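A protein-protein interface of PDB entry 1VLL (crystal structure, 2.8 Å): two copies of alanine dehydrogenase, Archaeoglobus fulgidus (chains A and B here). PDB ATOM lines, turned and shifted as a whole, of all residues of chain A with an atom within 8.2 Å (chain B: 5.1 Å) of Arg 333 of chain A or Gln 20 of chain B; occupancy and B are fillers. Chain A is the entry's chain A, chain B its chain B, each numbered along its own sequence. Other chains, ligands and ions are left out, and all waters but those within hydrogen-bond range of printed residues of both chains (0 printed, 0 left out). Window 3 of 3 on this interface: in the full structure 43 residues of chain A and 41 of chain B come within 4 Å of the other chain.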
ATOM      1  N   MET A  13     -16.964   7.780  -1.539  1.00  0.00           N
ATOM      2  CA  MET A  13     -15.825   8.544  -0.924  1.00  0.00           C
ATOM      3  C   MET A  13     -16.021   8.862   0.565  1.00  0.00           C
ATOM      4  O   MET A  13     -17.134   9.194   1.010  1.00  0.00           O
ATOM      5  CB  MET A  13     -15.519   9.837  -1.698  1.00  0.00           C
ATOM      6  CG  MET A  13     -14.528   9.655  -2.853  1.00  0.00           C
ATOM      7  SD  MET A  13     -14.256  11.138  -3.868  1.00  0.00           S
ATOM      8  CE  MET A  13     -14.427  10.435  -5.532  1.00  0.00           C
ATOM      9  N   ILE A 329     -13.876   8.491   8.057  1.00  0.00           N
ATOM     10  CA  ILE A 329     -15.206   9.003   8.432  1.00  0.00           C
ATOM     11  C   ILE A 329     -16.013   9.404   7.190  1.00  0.00           C
ATOM     12  O   ILE A 329     -15.494  10.073   6.296  1.00  0.00           O
ATOM     13  CB  ILE A 329     -15.114  10.175   9.467  1.00  0.00           C
ATOM     14  CG1 ILE A 329     -14.671   9.666  10.851  1.00  0.00           C
ATOM     15  CG2 ILE A 329     -16.424  10.942   9.574  1.00  0.00           C
ATOM     16  CD1 ILE A 329     -15.471   8.468  11.418  1.00  0.00           C
ATOM     17  N   LYS A 330     -17.267   8.954   7.127  1.00  0.00           N
ATOM     18  CA  LYS A 330     -18.155   9.300   6.020  1.00  0.00           C
ATOM     19  C   LYS A 330     -19.067  10.431   6.471  1.00  0.00           C
ATOM     20  O   LYS A 330     -20.080  10.195   7.140  1.00  0.00           O
ATOM     21  CB  LYS A 330     -18.961   8.080   5.533  1.00  0.00           C
ATOM     22  N   PHE A 331     -18.701  11.659   6.115  1.00  0.00           N
ATOM     23  CA  PHE A 331     -19.451  12.833   6.572  1.00  0.00           C
ATOM     24  C   PHE A 331     -20.818  13.014   5.929  1.00  0.00           C
ATOM     25  O   PHE A 331     -21.710  13.593   6.540  1.00  0.00           O
ATOM     26  CB  PHE A 331     -18.632  14.129   6.425  1.00  0.00           C
ATOM     27  CG  PHE A 331     -17.688  14.381   7.568  1.00  0.00           C
ATOM     28  CD1 PHE A 331     -18.176  14.631   8.851  1.00  0.00           C
ATOM     29  CD2 PHE A 331     -16.305  14.356   7.368  1.00  0.00           C
ATOM     30  CE1 PHE A 331     -17.303  14.846   9.920  1.00  0.00           C
ATOM     31  CE2 PHE A 331     -15.422  14.571   8.425  1.00  0.00           C
ATOM     32  CZ  PHE A 331     -15.923  14.818   9.707  1.00  0.00           C
ATOM     33  N   PHE A 332     -20.996  12.522   4.708  1.00  0.00           N
ATOM     34  CA  PHE A 332     -22.201  12.877   3.949  1.00  0.00           C
ATOM     35  C   PHE A 332     -23.051  11.724   3.380  1.00  0.00           C
ATOM     36  O   PHE A 332     -22.652  10.563   3.413  1.00  0.00           O
ATOM     37  CB  PHE A 332     -21.798  13.844   2.845  1.00  0.00           C
ATOM     38  CG  PHE A 332     -20.769  14.823   3.271  1.00  0.00           C
ATOM     39  CD1 PHE A 332     -21.109  15.895   4.086  1.00  0.00           C
ATOM     40  CD2 PHE A 332     -19.454  14.663   2.888  1.00  0.00           C
ATOM     41  CE1 PHE A 332     -20.147  16.809   4.494  1.00  0.00           C
ATOM     42  CE2 PHE A 332     -18.496  15.569   3.282  1.00  0.00           C
ATOM     43  CZ  PHE A 332     -18.842  16.649   4.087  1.00  0.00           C
ATOM     44  N   ARG A 333     -24.221  12.077   2.851  1.00  0.00           N
ATOM     45  CA  ARG A 333     -25.191  11.120   2.328  1.00  0.00           C
ATOM     46  C   ARG A 333     -25.376  11.297   0.825  1.00  0.00           C
ATOM     47  O   ARG A 333     -24.464  11.735   0.130  1.00  0.00           O
ATOM     48  CB  ARG A 333     -26.534  11.313   3.044  1.00  0.00           C
ATOM     49  N   LEU B  18     -19.155  14.444  14.265  1.00  0.00           N
ATOM     50  CA  LEU B  18     -20.543  14.100  13.987  1.00  0.00           C
ATOM     51  C   LEU B  18     -20.831  14.115  12.470  1.00  0.00           C
ATOM     52  O   LEU B  18     -20.528  15.099  11.799  1.00  0.00           O
ATOM     53  CB  LEU B  18     -21.476  15.050  14.763  1.00  0.00           C
ATOM     54  CG  LEU B  18     -21.499  15.012  16.304  1.00  0.00           C
ATOM     55  N   THR B  19     -21.401  13.029  11.935  1.00  0.00           N
ATOM     56  CA  THR B  19     -21.718  12.957  10.500  1.00  0.00           C
ATOM     57  C   THR B  19     -23.108  13.492  10.225  1.00  0.00           C
ATOM     58  O   THR B  19     -23.915  13.655  11.143  1.00  0.00           O
ATOM     59  CB  THR B  19     -21.695  11.526   9.943  1.00  0.00           C
ATOM     60  OG1 THR B  19     -22.951  10.893  10.221  1.00  0.00           O
ATOM     61  CG2 THR B  19     -20.550  10.712  10.529  1.00  0.00           C
ATOM     62  N   GLN B  20     -23.387  13.728   8.950  1.00  0.00           N
ATOM     63  CA  GLN B  20     -24.676  14.229   8.520  1.00  0.00           C
ATOM     64  C   GLN B  20     -25.835  13.507   9.224  1.00  0.00           C
ATOM     65  O   GLN B  20     -26.642  14.146   9.901  1.00  0.00           O
ATOM     66  CB  GLN B  20     -24.792  14.128   7.002  1.00  0.00           C
ATOM     67  CG  GLN B  20     -25.992  14.847   6.432  1.00  0.00           C
ATOM     68  CD  GLN B  20     -25.919  15.020   4.928  1.00  0.00           C
ATOM     69  OE1 GLN B  20     -24.939  14.647   4.275  1.00  0.00           O
ATOM     70  NE2 GLN B  20     -26.966  15.598   4.369  1.00  0.00           N
ATOM     71  N   GLU B  21     -25.888  12.184   9.088  1.00  0.00           N
ATOM     72  CA  GLU B  21     -26.903  11.364   9.759  1.00  0.00           C
ATOM     73  C   GLU B  21     -27.081  11.742  11.226  1.00  0.00           C
ATOM     74  O   GLU B  21     -28.198  11.976  11.690  1.00  0.00           O
ATOM     75  CB  GLU B  21     -26.525   9.885   9.688  1.00  0.00           C
ATOM     76  CG  GLU B  21     -27.041   9.133   8.469  1.00  0.00           C
ATOM     77  CD  GLU B  21     -26.761   7.629   8.564  1.00  0.00           C
ATOM     78  OE1 GLU B  21     -26.956   7.039   9.659  1.00  0.00           O
ATOM     79  OE2 GLU B  21     -26.347   7.037   7.537  1.00  0.00           O
ATOM     80  N   GLU B  22     -25.971  11.798  11.949  1.00  0.00           N
ATOM     81  CA  GLU B  22     -25.996  12.119  13.369  1.00  0.00           C
ATOM     82  C   GLU B  22     -26.581  13.513  13.637  1.00  0.00           C
ATOM     83  O   GLU B  22     -27.523  13.654  14.430  1.00  0.00           O
ATOM     84  CB  GLU B  22     -24.590  11.957  13.970  1.00  0.00           C
ATOM     85  CG  GLU B  22     -24.184  10.486  14.201  1.00  0.00           C
ATOM     86  CD  GLU B  22     -22.667  10.219  14.164  1.00  0.00           C
ATOM     87  OE1 GLU B  22     -21.884  11.055  13.646  1.00  0.00           O
ATOM     88  OE2 GLU B  22     -22.263   9.137  14.653  1.00  0.00           O
ATOM     89  N   VAL B  23     -26.051  14.522  12.948  1.00  0.00           N
ATOM     90  CA  VAL B  23     -26.515  15.910  13.096  1.00  0.00           C
ATOM     91  C   VAL B  23     -28.010  16.031  12.840  1.00  0.00           C
ATOM     92  O   VAL B  23     -28.717  16.718  13.579  1.00  0.00           O
ATOM     93  CB  VAL B  23     -25.740  16.901  12.177  1.00  0.00           C
ATOM     94  CG1 VAL B  23     -26.324  18.311  12.249  1.00  0.00           C
ATOM     95  CG2 VAL B  23     -24.262  16.936  12.552  1.00  0.00           C
ATOM     96  N   GLU B  24     -28.486  15.341  11.809  1.00  0.00           N
ATOM     97  CA  GLU B  24     -29.896  15.394  11.435  1.00  0.00           C
ATOM     98  C   GLU B  24     -30.808  15.153  12.619  1.00  0.00           C
ATOM     99  O   GLU B  24     -31.764  15.899  12.824  1.00  0.00           O
ATOM    100  CB  GLU B  24     -30.201  14.412  10.301  1.00  0.00           C
ATOM    101  CG  GLU B  24     -29.723  14.928   8.954  1.00  0.00           C
ATOM    102  CD  GLU B  24     -30.108  14.054   7.778  1.00  0.00           C
ATOM    103  OE1 GLU B  24     -30.914  13.096   7.935  1.00  0.00           O
ATOM    104  OE2 GLU B  24     -29.594  14.349   6.676  1.00  0.00           O
ATOM    105  N   PRO B  91     -22.564  15.618  -4.080  1.00  0.00           N
ATOM    106  CA  PRO B  91     -23.493  16.739  -3.927  1.00  0.00           C
ATOM    107  C   PRO B  91     -22.833  18.033  -4.368  1.00  0.00           C
ATOM    108  O   PRO B  91     -21.609  18.165  -4.263  1.00  0.00           O
ATOM    109  CB  PRO B  91     -23.759  16.774  -2.423  1.00  0.00           C
ATOM    110  CG  PRO B  91     -23.136  15.523  -1.865  1.00  0.00           C
ATOM    111  CD  PRO B  91     -22.046  15.163  -2.781  1.00  0.00           C
ATOM    112  N   ASP B 112     -20.664  17.694  10.195  1.00  0.00           N
ATOM    113  CA  ASP B 112     -21.253  18.095   8.925  1.00  0.00           C
ATOM    114  C   ASP B 112     -22.064  19.380   9.092  1.00  0.00           C
ATOM    115  O   ASP B 112     -22.735  19.589  10.125  1.00  0.00           O
ATOM    116  CB  ASP B 112     -22.154  17.007   8.344  1.00  0.00           C
ATOM    117  CG  ASP B 112     -23.168  17.567   7.339  1.00  0.00           C
ATOM    118  OD1 ASP B 112     -22.716  18.122   6.303  1.00  0.00           O
ATOM    119  OD2 ASP B 112     -24.401  17.471   7.605  1.00  0.00           O
ATOM    120  N   THR B 114     -23.602  20.511   5.987  1.00  0.00           N
ATOM    121  CA  THR B 114     -24.397  20.496   4.774  1.00  0.00           C
ATOM    122  C   THR B 114     -25.865  20.629   5.159  1.00  0.00           C
ATOM    123  O   THR B 114     -26.557  21.542   4.693  1.00  0.00           O
ATOM    124  CB  THR B 114     -24.197  19.197   3.997  1.00  0.00           C
ATOM    125  OG1 THR B 114     -22.820  18.803   4.081  1.00  0.00           O
ATOM    126  CG2 THR B 114     -24.619  19.371   2.528  1.00  0.00           C
ATOM    127  N   TYR B 115     -26.317  19.734   6.033  1.00  0.00           N
ATOM    128  CA  TYR B 115     -27.701  19.714   6.479  1.00  0.00           C
ATOM    129  C   TYR B 115     -28.068  20.977   7.235  1.00  0.00           C
ATOM    130  O   TYR B 115     -29.109  21.583   6.962  1.00  0.00           O
ATOM    131  CB  TYR B 115     -27.956  18.494   7.362  1.00  0.00           C
ATOM    132  CG  TYR B 115     -29.316  18.505   8.008  1.00  0.00           C
ATOM    133  CD1 TYR B 115     -30.440  18.151   7.288  1.00  0.00           C
ATOM    134  CD2 TYR B 115     -29.477  18.885   9.334  1.00  0.00           C
ATOM    135  CE1 TYR B 115     -31.687  18.168   7.866  1.00  0.00           C
ATOM    136  CE2 TYR B 115     -30.722  18.913   9.923  1.00  0.00           C
ATOM    137  CZ  TYR B 115     -31.827  18.551   9.184  1.00  0.00           C
ATOM    138  OH  TYR B 115     -33.085  18.555   9.752  1.00  0.00           O
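The backbone carbonyl oxygen (O) of Phe 331 of chain A sits at hydrogen-bond distance from the backbone NH (N) of Gln 20 of chain B, 2.9 Å away.
The backbone NH of Arg 333 of chain A is in hydrogen-bond range of the side-chain amide oxygen of Gln 20 of chain B.
O of Leu 18 of chain B is in hydrogen-bond range of N of Asp 112 of chain B (3.1 Å).
The backbone NH of Glu 21 of chain B sits close to the side-chain hydroxyl of Thr 19 of chain B.
The backbone NH (N) of Thr 19 of chain B lies within hydrogen-bond range of the side-chain carboxylate (OE1) of Glu 22 of chain B (2.7 Å).
N of Thr 114 of chain B lies within hydrogen-bond range of OD1 of Asp 112 of chain B (2.6 Å).
N of Tyr 115 of chain B is in hydrogen-bond range of OD2 of Asp 112 of chain B.
Among the printed residues, merely in contact across the chains: Lys 330 of chain A with Thr 19 of chain B, Phe 331 of chain A with Leu 18 of chain B, Phe 331 of chain A with Thr 19 of chain B, Phe 331 of chain A with Asp 112 of chain B, Phe 332 of chain A with Gln 20 of chain B, Phe 332 of chain A with Asp 112 of chain B and Phe 332 of chain A with Thr 114 of chain B.
Printed residues of chain B within 4 Å of Lys 330 of chain A: Thr 19 (3.5 Å).
Printed residues of chain B within 4 Å of Phe 332 of chain A: Gln 20, Asp 112 and Thr 114.
Printed residues of chain B within 4 Å of Arg 333 of chain A: Gln 20.
Of the printed residues of chain A, Leu 18 of chain B touches Phe 331.
Of the printed residues of chain A, Thr 19 of chain B touches Lys 330 and Phe 331.
Of chain A, only Phe 331 (2.9 Å), Phe 332 (3.3 Å) and Arg 333 (3.0 Å) come within 4 Å of Gln 20 of chain B.
The nearest residue of chain B that does not touch Arg 333 of chain A is Pro 91 of chain B (4.5 Å).
Printed residues of chain A that touch a printed residue of chain B: Lys 330, Phe 331, Phe 332 and Arg 333.
Hydrophobic or aromatic side chains of chain A within 4 Å of the printed part of chain B: Phe 331 and Phe 332.
Among the printed residues, 9 pairs touch across the chains.
No position is printed for both chains.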
